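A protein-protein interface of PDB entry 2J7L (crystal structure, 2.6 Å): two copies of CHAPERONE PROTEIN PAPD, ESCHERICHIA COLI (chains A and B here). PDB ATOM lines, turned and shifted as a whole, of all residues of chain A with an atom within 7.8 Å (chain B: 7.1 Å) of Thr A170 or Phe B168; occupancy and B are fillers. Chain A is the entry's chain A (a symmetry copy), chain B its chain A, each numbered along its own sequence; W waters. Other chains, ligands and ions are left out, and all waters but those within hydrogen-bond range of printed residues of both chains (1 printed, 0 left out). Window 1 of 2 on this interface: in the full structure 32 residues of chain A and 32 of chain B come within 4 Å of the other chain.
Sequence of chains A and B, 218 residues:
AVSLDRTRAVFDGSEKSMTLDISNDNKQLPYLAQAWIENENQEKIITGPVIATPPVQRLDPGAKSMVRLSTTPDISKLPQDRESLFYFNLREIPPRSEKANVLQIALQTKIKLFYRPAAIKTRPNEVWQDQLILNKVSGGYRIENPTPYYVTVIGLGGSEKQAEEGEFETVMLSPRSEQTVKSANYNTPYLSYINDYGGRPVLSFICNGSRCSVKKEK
Among the printed residues, merely in contact across the chains: Thr A152 with Glu B167 (3.4 Å), Glu A167 with Thr B152 (3.4 Å), Glu A167 with Thr B170 (3.5 Å), Thr A170 with Glu B167 (3.5 Å), Arg A200 with Gly B166 (3.7 Å), Ile A194 with Glu B165 (3.9 Å) and Ile A194 with Glu B167 (3.9 Å).
Of the printed residues of chain B, Lys A112 touches Glu B167. Thr A170 touches just these residues of chain B: Glu B167 and Phe B168. Of the printed residues of chain B, Ile A194 touches Glu B165 (3.9 Å) and Glu B167 (3.9 Å). Printed residues of chain B within 4 Å of Arg A200: Glu B165 and Gly B166. Leu B156 touches none of the printed residues of chain A. Of the printed residues of chain A, Phe B168 touches Thr A170. Printed residues of chain A within 4 Å of Glu B169: Glu A169. Of the printed residues of chain A, Thr B170 touches Glu A167 (3.5 Å) and Phe A168 (3.1 Å). Val B171 touches none of the printed residues of chain A. The nearest residue of chain B that does not touch Thr A170 is Glu B169 (4.4 Å). The nearest printed residue of chain A that does not touch Glu B169 is Thr A170 (4.4 Å).
Water W1 lies within hydrogen-bond range of the backbone carbonyl oxygen of Gly B166 (2.6 Å), the guanidinium group of Arg A200 (2.9 Å), the backbone carbonyl oxygen of Ile B154 (3.3 Å) and the backbone NH of Phe B168 (3.3 Å).
The side-chain carboxylate of Glu B167 is in salt-bridge range of the side-chain amino group of Lys A112, 3.1 Å away. The backbone carbonyl oxygen (O) of Glu B165 lies within hydrogen-bond range of the guanidinium group (NH1) of Arg A200, at 3.0 Å. OE1 of Glu B169 sits close to OE1 of Glu A169, 2.7 Å away. The backbone carbonyl oxygen of Phe B168 sits at hydrogen-bond distance from the side-chain hydroxyl of Thr A170 (3.1 Å). The side-chain hydroxyl of Thr B170 sits at hydrogen-bond distance from the backbone carbonyl oxygen of Phe A168 (3.1 Å).
The backbone NH (N) of Ile A194 lies within hydrogen-bond range of the backbone carbonyl oxygen (O) of Thr A152 (3.1 Å).
Thr A152 touches Glu B167, and with the chains exchanged Glu A167 touches Thr B152. Glu A167 touches Thr B170, and with the chains exchanged Thr A170 touches Glu B167. Phe A168 touches Thr B170, and with the chains exchanged Thr A170 touches Phe B168. Glu B169 touches its own counterpart, Glu A169. Positions printed for both chains: 152, 153, 154, 155, 167, 168, 169, 170, 171, 181 and 192. Of the 12 pairs that touch across the chains among the printed residues, 7 have their exchanged pair printed and touching as well.
Of the 18 printed residues of chain A, 8 touch a printed residue of chain B. Printed residues of chain A that touch a printed residue of chain B: Lys A112, Thr A152, Glu A167, Phe A168, Glu A169, Thr A170, Ile A194 and Arg A200. Hydrophobic or aromatic side chains of chain A that line the printed part of chain B: Ile A194. Along chain A the printed residues that touch a printed residue of chain B span positions 112 to 200. Of the 21 printed residues of chain B, 7 touch a printed residue of chain A. Among the printed residues, 12 pairs touch across the chains. Among the printed residues, Asp or Glu carboxylates within 4 Å of a Lys or Arg side-chain nitrogen of the other chain: Lys A112 with Glu B167 (3.1 Å).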
ATOM      1  N   LYS A 112      -7.061 -14.419  -9.680  1.00  0.00           N
ATOM      2  CA  LYS A 112      -6.552 -14.956  -8.440  1.00  0.00           C
ATOM      3  C   LYS A 112      -7.054 -14.079  -7.295  1.00  0.00           C
ATOM      4  O   LYS A 112      -7.259 -12.866  -7.445  1.00  0.00           O
ATOM      5  CB  LYS A 112      -5.016 -15.001  -8.456  1.00  0.00           C
ATOM      6  CG  LYS A 112      -4.428 -16.054  -9.390  1.00  0.00           C
ATOM      7  CD  LYS A 112      -2.904 -16.097  -9.326  1.00  0.00           C
ATOM      8  CE  LYS A 112      -2.328 -17.296 -10.072  1.00  0.00           C
ATOM      9  NZ  LYS A 112      -2.647 -17.241 -11.520  1.00  0.00           N
ATOM     10  N   VAL A 151       4.395 -14.129  -4.854  1.00  0.00           N
ATOM     11  CA  VAL A 151       5.086 -13.214  -5.747  1.00  0.00           C
ATOM     12  C   VAL A 151       5.041 -13.802  -7.142  1.00  0.00           C
ATOM     13  O   VAL A 151       5.468 -14.946  -7.373  1.00  0.00           O
ATOM     14  CB  VAL A 151       6.564 -13.014  -5.352  1.00  0.00           C
ATOM     15  CG1 VAL A 151       7.231 -12.038  -6.323  1.00  0.00           C
ATOM     16  CG2 VAL A 151       6.652 -12.501  -3.922  1.00  0.00           C
ATOM     17  N   THR A 152       4.515 -13.007  -8.067  1.00  0.00           N
ATOM     18  CA  THR A 152       4.389 -13.422  -9.454  1.00  0.00           C
ATOM     19  C   THR A 152       5.400 -12.659 -10.312  1.00  0.00           C
ATOM     20  O   THR A 152       5.383 -11.427 -10.362  1.00  0.00           O
ATOM     21  CB  THR A 152       2.940 -13.169  -9.959  1.00  0.00           C
ATOM     22  OG1 THR A 152       2.008 -13.819  -9.080  1.00  0.00           O
ATOM     23  CG2 THR A 152       2.754 -13.707 -11.364  1.00  0.00           C
ATOM     24  N   VAL A 153       6.284 -13.409 -10.975  1.00  0.00           N
ATOM     25  CA  VAL A 153       7.325 -12.839 -11.840  1.00  0.00           C
ATOM     26  C   VAL A 153       6.943 -13.014 -13.319  1.00  0.00           C
ATOM     27  O   VAL A 153       6.833 -14.145 -13.793  1.00  0.00           O
ATOM     28  CB  VAL A 153       8.696 -13.537 -11.605  1.00  0.00           C
ATOM     29  CG1 VAL A 153       9.763 -12.928 -12.503  1.00  0.00           C
ATOM     30  CG2 VAL A 153       9.089 -13.431 -10.153  1.00  0.00           C
ATOM     31  N   ILE A 154       6.746 -11.895 -14.027  1.00  0.00           N
ATOM     32  CA  ILE A 154       6.383 -11.915 -15.450  1.00  0.00           C
ATOM     33  C   ILE A 154       7.498 -11.428 -16.387  1.00  0.00           C
ATOM     34  O   ILE A 154       7.362 -11.472 -17.606  1.00  0.00           O
ATOM     35  CB  ILE A 154       5.090 -11.073 -15.740  1.00  0.00           C
ATOM     36  CG1 ILE A 154       5.087  -9.783 -14.919  1.00  0.00           C
ATOM     37  CG2 ILE A 154       3.851 -11.868 -15.410  1.00  0.00           C
ATOM     38  CD1 ILE A 154       5.980  -8.715 -15.463  1.00  0.00           C
ATOM     39  N   GLY A 155       8.613 -10.980 -15.828  1.00  0.00           N
ATOM     40  CA  GLY A 155       9.691 -10.504 -16.673  1.00  0.00           C
ATOM     41  C   GLY A 155      11.064 -10.742 -16.095  1.00  0.00           C
ATOM     42  O   GLY A 155      11.249 -10.808 -14.883  1.00  0.00           O
ATOM     43  N   GLU A 167      10.111 -11.685 -23.689  1.00  0.00           N
ATOM     44  CA  GLU A 167       9.218 -12.796 -23.386  1.00  0.00           C
ATOM     45  C   GLU A 167       9.780 -13.640 -22.252  1.00  0.00           C
ATOM     46  O   GLU A 167      10.964 -13.962 -22.226  1.00  0.00           O
ATOM     47  CB  GLU A 167       9.019 -13.639 -24.647  1.00  0.00           C
ATOM     48  CG  GLU A 167      10.279 -13.781 -25.472  1.00  0.00           C
ATOM     49  CD  GLU A 167       9.992 -13.995 -26.946  1.00  0.00           C
ATOM     50  OE1 GLU A 167       9.827 -15.162 -27.367  1.00  0.00           O
ATOM     51  OE2 GLU A 167       9.923 -12.988 -27.682  1.00  0.00           O
ATOM     52  N   PHE A 168       8.919 -13.996 -21.310  1.00  0.00           N
ATOM     53  CA  PHE A 168       9.338 -14.774 -20.151  1.00  0.00           C
ATOM     54  C   PHE A 168       8.213 -15.715 -19.717  1.00  0.00           C
ATOM     55  O   PHE A 168       7.024 -15.386 -19.832  1.00  0.00           O
ATOM     56  CB  PHE A 168       9.708 -13.799 -19.017  1.00  0.00           C
ATOM     57  CG  PHE A 168      10.063 -14.465 -17.721  1.00  0.00           C
ATOM     58  CD1 PHE A 168      11.218 -15.227 -17.604  1.00  0.00           C
ATOM     59  CD2 PHE A 168       9.220 -14.359 -16.624  1.00  0.00           C
ATOM     60  CE1 PHE A 168      11.527 -15.880 -16.412  1.00  0.00           C
ATOM     61  CE2 PHE A 168       9.511 -14.999 -15.434  1.00  0.00           C
ATOM     62  CZ  PHE A 168      10.670 -15.767 -15.324  1.00  0.00           C
ATOM     63  N   GLU A 169       8.583 -16.890 -19.225  1.00  0.00           N
ATOM     64  CA  GLU A 169       7.579 -17.837 -18.766  1.00  0.00           C
ATOM     65  C   GLU A 169       7.176 -17.475 -17.349  1.00  0.00           C
ATOM     66  O   GLU A 169       7.863 -17.816 -16.392  1.00  0.00           O
ATOM     67  CB  GLU A 169       8.125 -19.257 -18.809  1.00  0.00           C
ATOM     68  CG  GLU A 169       7.224 -20.274 -18.152  1.00  0.00           C
ATOM     69  CD  GLU A 169       7.612 -21.696 -18.501  1.00  0.00           C
ATOM     70  OE1 GLU A 169       7.021 -22.636 -17.918  1.00  0.00           O
ATOM     71  OE2 GLU A 169       8.505 -21.868 -19.365  1.00  0.00           O
ATOM     72  N   THR A 170       6.063 -16.766 -17.225  1.00  0.00           N
ATOM     73  CA  THR A 170       5.570 -16.336 -15.926  1.00  0.00           C
ATOM     74  C   THR A 170       5.572 -17.439 -14.889  1.00  0.00           C
ATOM     75  O   THR A 170       5.230 -18.579 -15.188  1.00  0.00           O
ATOM     76  CB  THR A 170       4.144 -15.795 -16.027  1.00  0.00           C
ATOM     77  OG1 THR A 170       4.129 -14.656 -16.895  1.00  0.00           O
ATOM     78  CG2 THR A 170       3.629 -15.397 -14.653  1.00  0.00           C
ATOM     79  N   VAL A 171       5.940 -17.081 -13.663  1.00  0.00           N
ATOM     80  CA  VAL A 171       5.978 -18.029 -12.555  1.00  0.00           C
ATOM     81  C   VAL A 171       5.500 -17.374 -11.258  1.00  0.00           C
ATOM     82  O   VAL A 171       5.793 -16.204 -10.986  1.00  0.00           O
ATOM     83  CB  VAL A 171       7.416 -18.589 -12.358  1.00  0.00           C
ATOM     84  CG1 VAL A 171       8.397 -17.448 -12.109  1.00  0.00           C
ATOM     85  CG2 VAL A 171       7.440 -19.571 -11.203  1.00  0.00           C
ATOM     86  N   MET A 172       4.743 -18.119 -10.463  1.00  0.00           N
ATOM     87  CA  MET A 172       4.261 -17.582  -9.203  1.00  0.00           C
ATOM     88  C   MET A 172       4.853 -18.343  -8.030  1.00  0.00           C
ATOM     89  O   MET A 172       4.550 -19.511  -7.820  1.00  0.00           O
ATOM     90  CB  MET A 172       2.741 -17.648  -9.124  1.00  0.00           C
ATOM     91  CG  MET A 172       2.195 -17.144  -7.810  1.00  0.00           C
ATOM     92  SD  MET A 172       0.409 -17.237  -7.824  1.00  0.00           S
ATOM     93  CE  MET A 172       0.170 -18.972  -7.414  1.00  0.00           C
ATOM     94  N   LEU A 173       5.690 -17.660  -7.259  1.00  0.00           N
ATOM     95  CA  LEU A 173       6.337 -18.269  -6.109  1.00  0.00           C
ATOM     96  C   LEU A 173       5.440 -18.188  -4.880  1.00  0.00           C
ATOM     97  O   LEU A 173       4.931 -17.117  -4.526  1.00  0.00           O
ATOM     98  CB  LEU A 173       7.664 -17.564  -5.849  1.00  0.00           C
ATOM     99  CG  LEU A 173       8.531 -17.305  -7.089  1.00  0.00           C
ATOM    100  CD1 LEU A 173       9.631 -16.348  -6.722  1.00  0.00           C
ATOM    101  CD2 LEU A 173       9.109 -18.593  -7.634  1.00  0.00           C
ATOM    102  N   GLN A 179      11.819 -21.377  -6.561  1.00  0.00           N
ATOM    103  CA  GLN A 179      11.616 -22.075  -7.821  1.00  0.00           C
ATOM    104  C   GLN A 179      12.719 -21.765  -8.810  1.00  0.00           C
ATOM    105  O   GLN A 179      13.337 -20.709  -8.752  1.00  0.00           O
ATOM    106  CB  GLN A 179      10.289 -21.712  -8.446  1.00  0.00           C
ATOM    107  CG  GLN A 179       9.130 -21.939  -7.538  1.00  0.00           C
ATOM    108  CD  GLN A 179       7.875 -22.117  -8.319  1.00  0.00           C
ATOM    109  OE1 GLN A 179       6.774 -21.905  -7.804  1.00  0.00           O
ATOM    110  NE2 GLN A 179       8.020 -22.525  -9.577  1.00  0.00           N
ATOM    111  N   VAL A 181      13.750 -21.163 -12.693  1.00  0.00           N
ATOM    112  CA  VAL A 181      13.243 -20.738 -13.987  1.00  0.00           C
ATOM    113  C   VAL A 181      14.338 -20.783 -15.049  1.00  0.00           C
ATOM    114  O   VAL A 181      15.520 -20.883 -14.726  1.00  0.00           O
ATOM    115  CB  VAL A 181      12.698 -19.309 -13.880  1.00  0.00           C
ATOM    116  CG1 VAL A 181      11.739 -19.232 -12.716  1.00  0.00           C
ATOM    117  CG2 VAL A 181      13.844 -18.321 -13.690  1.00  0.00           C
ATOM    118  N   SER A 192      10.744  -8.340 -13.195  1.00  0.00           N
ATOM    119  CA  SER A 192       9.479  -7.651 -13.328  1.00  0.00           C
ATOM    120  C   SER A 192       8.400  -8.523 -12.699  1.00  0.00           C
ATOM    121  O   SER A 192       8.290  -9.711 -13.005  1.00  0.00           O
ATOM    122  CB  SER A 192       9.183  -7.406 -14.799  1.00  0.00           C
ATOM    123  OG  SER A 192       8.024  -6.615 -14.935  1.00  0.00           O
ATOM    124  N   ILE A 194       4.181  -8.646 -10.731  1.00  0.00           N
ATOM    125  CA  ILE A 194       2.844  -8.071 -10.740  1.00  0.00           C
ATOM    126  C   ILE A 194       2.426  -7.703  -9.311  1.00  0.00           C
ATOM    127  O   ILE A 194       2.429  -8.545  -8.413  1.00  0.00           O
ATOM    128  CB  ILE A 194       1.806  -9.059 -11.328  1.00  0.00           C
ATOM    129  CG1 ILE A 194       2.234  -9.509 -12.733  1.00  0.00           C
ATOM    130  CG2 ILE A 194       0.440  -8.384 -11.385  1.00  0.00           C
ATOM    131  CD1 ILE A 194       1.368 -10.601 -13.335  1.00  0.00           C
ATOM    132  N   ARG A 200       3.031  -3.728 -13.279  1.00  0.00           N
ATOM    133  CA  ARG A 200       4.212  -4.502 -13.644  1.00  0.00           C
ATOM    134  C   ARG A 200       5.531  -3.790 -13.303  1.00  0.00           C
ATOM    135  O   ARG A 200       6.320  -3.471 -14.191  1.00  0.00           O
ATOM    136  CB  ARG A 200       4.178  -4.823 -15.139  1.00  0.00           C
ATOM    137  CG  ARG A 200       3.362  -6.050 -15.520  1.00  0.00           C
ATOM    138  CD  ARG A 200       3.259  -6.193 -17.040  1.00  0.00           C
ATOM    139  NE  ARG A 200       3.030  -7.571 -17.487  1.00  0.00           N
ATOM    140  CZ  ARG A 200       1.975  -8.317 -17.167  1.00  0.00           C
ATOM    141  NH1 ARG A 200       1.025  -7.823 -16.381  1.00  0.00           N
ATOM    142  NH2 ARG A 200       1.866  -9.554 -17.644  1.00  0.00           N
ATOM    143  N   ILE B 143      -3.148 -23.821 -30.052  1.00  0.00           N
ATOM    144  CA  ILE B 143      -2.971 -22.724 -30.998  1.00  0.00           C
ATOM    145  C   ILE B 143      -2.290 -23.158 -32.290  1.00  0.00           C
ATOM    146  O   ILE B 143      -1.322 -23.916 -32.269  1.00  0.00           O
ATOM    147  CB  ILE B 143      -2.154 -21.582 -30.370  1.00  0.00           C
ATOM    148  CG1 ILE B 143      -2.731 -21.244 -28.993  1.00  0.00           C
ATOM    149  CG2 ILE B 143      -2.150 -20.368 -31.304  1.00  0.00           C
ATOM    150  CD1 ILE B 143      -2.053 -20.092 -28.289  1.00  0.00           C
ATOM    151  N   THR B 152       4.792 -14.997 -31.447  1.00  0.00           N
ATOM    152  CA  THR B 152       5.011 -15.106 -30.015  1.00  0.00           C
ATOM    153  C   THR B 152       3.776 -14.597 -29.267  1.00  0.00           C
ATOM    154  O   THR B 152       3.374 -13.443 -29.425  1.00  0.00           O
ATOM    155  CB  THR B 152       6.273 -14.297 -29.602  1.00  0.00           C
ATOM    156  OG1 THR B 152       7.395 -14.730 -30.386  1.00  0.00           O
ATOM    157  CG2 THR B 152       6.588 -14.495 -28.132  1.00  0.00           C
ATOM    158  N   VAL B 153       3.179 -15.480 -28.462  1.00  0.00           N
ATOM    159  CA  VAL B 153       1.982 -15.159 -27.674  1.00  0.00           C
ATOM    160  C   VAL B 153       2.356 -14.943 -26.199  1.00  0.00           C
ATOM    161  O   VAL B 153       2.828 -15.874 -25.546  1.00  0.00           O
ATOM    162  CB  VAL B 153       0.936 -16.309 -27.748  1.00  0.00           C
ATOM    163  CG1 VAL B 153      -0.301 -15.955 -26.935  1.00  0.00           C
ATOM    164  CG2 VAL B 153       0.572 -16.588 -29.185  1.00  0.00           C
ATOM    165  N   ILE B 154       2.142 -13.722 -25.695  1.00  0.00           N
ATOM    166  CA  ILE B 154       2.448 -13.378 -24.301  1.00  0.00           C
ATOM    167  C   ILE B 154       1.206 -13.147 -23.426  1.00  0.00           C
ATOM    168  O   ILE B 154       1.314 -12.938 -22.221  1.00  0.00           O
ATOM    169  CB  ILE B 154       3.371 -12.113 -24.195  1.00  0.00           C
ATOM    170  CG1 ILE B 154       2.961 -11.055 -25.220  1.00  0.00           C
ATOM    171  CG2 ILE B 154       4.815 -12.485 -24.423  1.00  0.00           C
ATOM    172  CD1 ILE B 154       1.743 -10.277 -24.837  1.00  0.00           C
ATOM    173  N   GLY B 155       0.024 -13.204 -24.019  1.00  0.00           N
ATOM    174  CA  GLY B 155      -1.176 -12.986 -23.235  1.00  0.00           C
ATOM    175  C   GLY B 155      -2.370 -13.768 -23.724  1.00  0.00           C
ATOM    176  O   GLY B 155      -2.487 -14.095 -24.901  1.00  0.00           O
ATOM    177  N   LEU B 156      -3.275 -14.080 -22.816  1.00  0.00           N
ATOM    178  CA  LEU B 156      -4.451 -14.821 -23.201  1.00  0.00           C
ATOM    179  C   LEU B 156      -5.414 -14.796 -22.047  1.00  0.00           C
ATOM    180  O   LEU B 156      -5.196 -15.463 -21.048  1.00  0.00           O
ATOM    181  CB  LEU B 156      -4.071 -16.254 -23.548  1.00  0.00           C
ATOM    182  CG  LEU B 156      -5.220 -17.189 -23.932  1.00  0.00           C
ATOM    183  CD1 LEU B 156      -6.099 -16.535 -24.979  1.00  0.00           C
ATOM    184  CD2 LEU B 156      -4.655 -18.502 -24.449  1.00  0.00           C
ATOM    185  N   GLY B 157      -6.468 -14.003 -22.185  1.00  0.00           N
ATOM    186  CA  GLY B 157      -7.463 -13.895 -21.135  1.00  0.00           C
ATOM    187  C   GLY B 157      -8.899 -13.829 -21.631  1.00  0.00           C
ATOM    188  O   GLY B 157      -9.171 -13.893 -22.828  1.00  0.00           O
ATOM    189  N   GLN B 162      -7.318  -8.360 -19.370  1.00  0.00           N
ATOM    190  CA  GLN B 162      -6.755  -9.571 -18.790  1.00  0.00           C
ATOM    191  C   GLN B 162      -5.663 -10.141 -19.680  1.00  0.00           C
ATOM    192  O   GLN B 162      -4.677 -10.682 -19.193  1.00  0.00           O
ATOM    193  CB  GLN B 162      -7.839 -10.629 -18.551  1.00  0.00           C
ATOM    194  CG  GLN B 162      -7.304 -11.849 -17.807  1.00  0.00           C
ATOM    195  CD  GLN B 162      -8.380 -12.790 -17.313  1.00  0.00           C
ATOM    196  OE1 GLN B 162      -9.158 -13.330 -18.091  1.00  0.00           O
ATOM    197  NE2 GLN B 162      -8.416 -13.002 -16.006  1.00  0.00           N
ATOM    198  N   ALA B 163      -5.838 -10.022 -20.989  1.00  0.00           N
ATOM    199  CA  ALA B 163      -4.837 -10.515 -21.915  1.00  0.00           C
ATOM    200  C   ALA B 163      -3.580  -9.656 -21.791  1.00  0.00           C
ATOM    201  O   ALA B 163      -2.548  -9.980 -22.356  1.00  0.00           O
ATOM    202  CB  ALA B 163      -5.375 -10.472 -23.337  1.00  0.00           C
ATOM    203  N   GLU B 165      -2.819  -7.591 -18.476  1.00  0.00           N
ATOM    204  CA  GLU B 165      -2.435  -7.646 -17.070  1.00  0.00           C
ATOM    205  C   GLU B 165      -2.294  -9.064 -16.543  1.00  0.00           C
ATOM    206  O   GLU B 165      -1.503  -9.312 -15.634  1.00  0.00           O
ATOM    207  CB  GLU B 165      -3.463  -6.897 -16.220  1.00  0.00           C
ATOM    208  CG  GLU B 165      -3.275  -5.388 -16.170  1.00  0.00           C
ATOM    209  CD  GLU B 165      -4.335  -4.693 -15.329  1.00  0.00           C
ATOM    210  OE1 GLU B 165      -4.682  -5.224 -14.248  1.00  0.00           O
ATOM    211  OE2 GLU B 165      -4.816  -3.615 -15.746  1.00  0.00           O
ATOM    212  N   GLY B 166      -3.067  -9.987 -17.109  1.00  0.00           N
ATOM    213  CA  GLY B 166      -3.026 -11.375 -16.674  1.00  0.00           C
ATOM    214  C   GLY B 166      -1.718 -12.087 -16.969  1.00  0.00           C
ATOM    215  O   GLY B 166      -1.026 -11.782 -17.948  1.00  0.00           O
ATOM    216  N   GLU B 167      -1.379 -13.043 -16.111  1.00  0.00           N
ATOM    217  CA  GLU B 167      -0.155 -13.821 -16.249  1.00  0.00           C
ATOM    218  C   GLU B 167      -0.363 -14.982 -17.208  1.00  0.00           C
ATOM    219  O   GLU B 167      -1.367 -15.686 -17.144  1.00  0.00           O
ATOM    220  CB  GLU B 167       0.281 -14.322 -14.871  1.00  0.00           C
ATOM    221  CG  GLU B 167      -0.881 -14.741 -13.997  1.00  0.00           C
ATOM    222  CD  GLU B 167      -0.581 -14.595 -12.517  1.00  0.00           C
ATOM    223  OE1 GLU B 167      -0.044 -15.548 -11.911  1.00  0.00           O
ATOM    224  OE2 GLU B 167      -0.879 -13.516 -11.963  1.00  0.00           O
ATOM    225  N   PHE B 168       0.594 -15.179 -18.102  1.00  0.00           N
ATOM    226  CA  PHE B 168       0.498 -16.236 -19.101  1.00  0.00           C
ATOM    227  C   PHE B 168       1.887 -16.799 -19.404  1.00  0.00           C
ATOM    228  O   PHE B 168       2.891 -16.073 -19.381  1.00  0.00           O
ATOM    229  CB  PHE B 168      -0.147 -15.649 -20.371  1.00  0.00           C
ATOM    230  CG  PHE B 168      -0.217 -16.604 -21.526  1.00  0.00           C
ATOM    231  CD1 PHE B 168      -1.042 -17.720 -21.479  1.00  0.00           C
ATOM    232  CD2 PHE B 168       0.573 -16.404 -22.650  1.00  0.00           C
ATOM    233  CE1 PHE B 168      -1.076 -18.629 -22.535  1.00  0.00           C
ATOM    234  CE2 PHE B 168       0.550 -17.295 -23.706  1.00  0.00           C
ATOM    235  CZ  PHE B 168      -0.276 -18.417 -23.651  1.00  0.00           C
ATOM    236  N   GLU B 169       1.951 -18.095 -19.680  1.00  0.00           N
ATOM    237  CA  GLU B 169       3.230 -18.710 -20.003  1.00  0.00           C
ATOM    238  C   GLU B 169       3.528 -18.475 -21.472  1.00  0.00           C
ATOM    239  O   GLU B 169       3.026 -19.184 -22.337  1.00  0.00           O
ATOM    240  CB  GLU B 169       3.196 -20.202 -19.705  1.00  0.00           C
ATOM    241  CG  GLU B 169       4.407 -20.948 -20.209  1.00  0.00           C
ATOM    242  CD  GLU B 169       4.513 -22.338 -19.615  1.00  0.00           C
ATOM    243  OE1 GLU B 169       5.404 -23.106 -20.049  1.00  0.00           O
ATOM    244  OE2 GLU B 169       3.706 -22.654 -18.708  1.00  0.00           O
ATOM    245  N   THR B 170       4.338 -17.463 -21.746  1.00  0.00           N
ATOM    246  CA  THR B 170       4.695 -17.116 -23.113  1.00  0.00           C
ATOM    247  C   THR B 170       5.098 -18.313 -23.949  1.00  0.00           C
ATOM    248  O   THR B 170       5.796 -19.202 -23.473  1.00  0.00           O
ATOM    249  CB  THR B 170       5.851 -16.116 -23.146  1.00  0.00           C
ATOM    250  OG1 THR B 170       5.453 -14.910 -22.483  1.00  0.00           O
ATOM    251  CG2 THR B 170       6.241 -15.804 -24.582  1.00  0.00           C
ATOM    252  N   VAL B 171       4.666 -18.312 -25.206  1.00  0.00           N
ATOM    253  CA  VAL B 171       4.984 -19.388 -26.138  1.00  0.00           C
ATOM    254  C   VAL B 171       5.250 -18.838 -27.540  1.00  0.00           C
ATOM    255  O   VAL B 171       4.586 -17.900 -27.996  1.00  0.00           O
ATOM    256  CB  VAL B 171       3.827 -20.427 -26.195  1.00  0.00           C
ATOM    257  CG1 VAL B 171       2.525 -19.744 -26.603  1.00  0.00           C
ATOM    258  CG2 VAL B 171       4.171 -21.538 -27.168  1.00  0.00           C
ATOM    259  N   VAL B 181      -1.269 -24.897 -25.246  1.00  0.00           N
ATOM    260  CA  VAL B 181      -0.974 -24.115 -24.058  1.00  0.00           C
ATOM    261  C   VAL B 181      -2.020 -24.348 -22.971  1.00  0.00           C
ATOM    262  O   VAL B 181      -3.088 -24.896 -23.238  1.00  0.00           O
ATOM    263  CB  VAL B 181      -0.943 -22.625 -24.419  1.00  0.00           C
ATOM    264  CG1 VAL B 181      -0.032 -22.425 -25.607  1.00  0.00           C
ATOM    265  CG2 VAL B 181      -2.349 -22.131 -24.738  1.00  0.00           C
ATOM    266  N   LYS B 182      -1.706 -23.947 -21.743  1.00  0.00           N
ATOM    267  CA  LYS B 182      -2.643 -24.114 -20.638  1.00  0.00           C
ATOM    268  C   LYS B 182      -3.388 -22.817 -20.401  1.00  0.00           C
ATOM    269  O   LYS B 182      -2.790 -21.745 -20.376  1.00  0.00           O
ATOM    270  CB  LYS B 182      -1.920 -24.528 -19.356  1.00  0.00           C
ATOM    271  CG  LYS B 182      -1.654 -26.013 -19.237  1.00  0.00           C
ATOM    272  CD  LYS B 182      -2.106 -26.537 -17.872  1.00  0.00           C
ATOM    273  CE  LYS B 182      -1.319 -25.890 -16.730  1.00  0.00           C
ATOM    274  NZ  LYS B 182      -1.859 -26.214 -15.365  1.00  0.00           N
ATOM    275  N   SER B 183      -4.698 -22.928 -20.218  1.00  0.00           N
ATOM    276  CA  SER B 183      -5.549 -21.768 -20.000  1.00  0.00           C
ATOM    277  C   SER B 183      -6.934 -22.186 -19.524  1.00  0.00           C
ATOM    278  O   SER B 183      -7.316 -23.349 -19.631  1.00  0.00           O
ATOM    279  CB  SER B 183      -5.682 -20.989 -21.307  1.00  0.00           C
ATOM    280  OG  SER B 183      -6.546 -19.875 -21.167  1.00  0.00           O
ATOM    281  N   LEU B 191      -6.282 -12.633 -27.195  1.00  0.00           N
ATOM    282  CA  LEU B 191      -4.900 -13.010 -27.408  1.00  0.00           C
ATOM    283  C   LEU B 191      -4.014 -11.782 -27.491  1.00  0.00           C
ATOM    284  O   LEU B 191      -4.417 -10.734 -27.980  1.00  0.00           O
ATOM    285  CB  LEU B 191      -4.796 -13.833 -28.699  1.00  0.00           C
ATOM    286  CG  LEU B 191      -3.673 -14.837 -28.958  1.00  0.00           C
ATOM    287  CD1 LEU B 191      -2.352 -14.108 -29.080  1.00  0.00           C
ATOM    288  CD2 LEU B 191      -3.638 -15.859 -27.848  1.00  0.00           C
ATOM    289  N   SER B 192      -2.797 -11.923 -26.993  1.00  0.00           N
ATOM    290  CA  SER B 192      -1.845 -10.835 -27.016  1.00  0.00           C
ATOM    291  C   SER B 192      -0.516 -11.383 -27.521  1.00  0.00           C
ATOM    292  O   SER B 192      -0.019 -12.394 -27.024  1.00  0.00           O
ATOM    293  CB  SER B 192      -1.693 -10.261 -25.617  1.00  0.00           C
ATOM    294  OG  SER B 192      -0.874  -9.113 -25.650  1.00  0.00           O
HETATM  295  O   HOH W   1       1.304 -12.061 -19.017  1.00  0.00           O
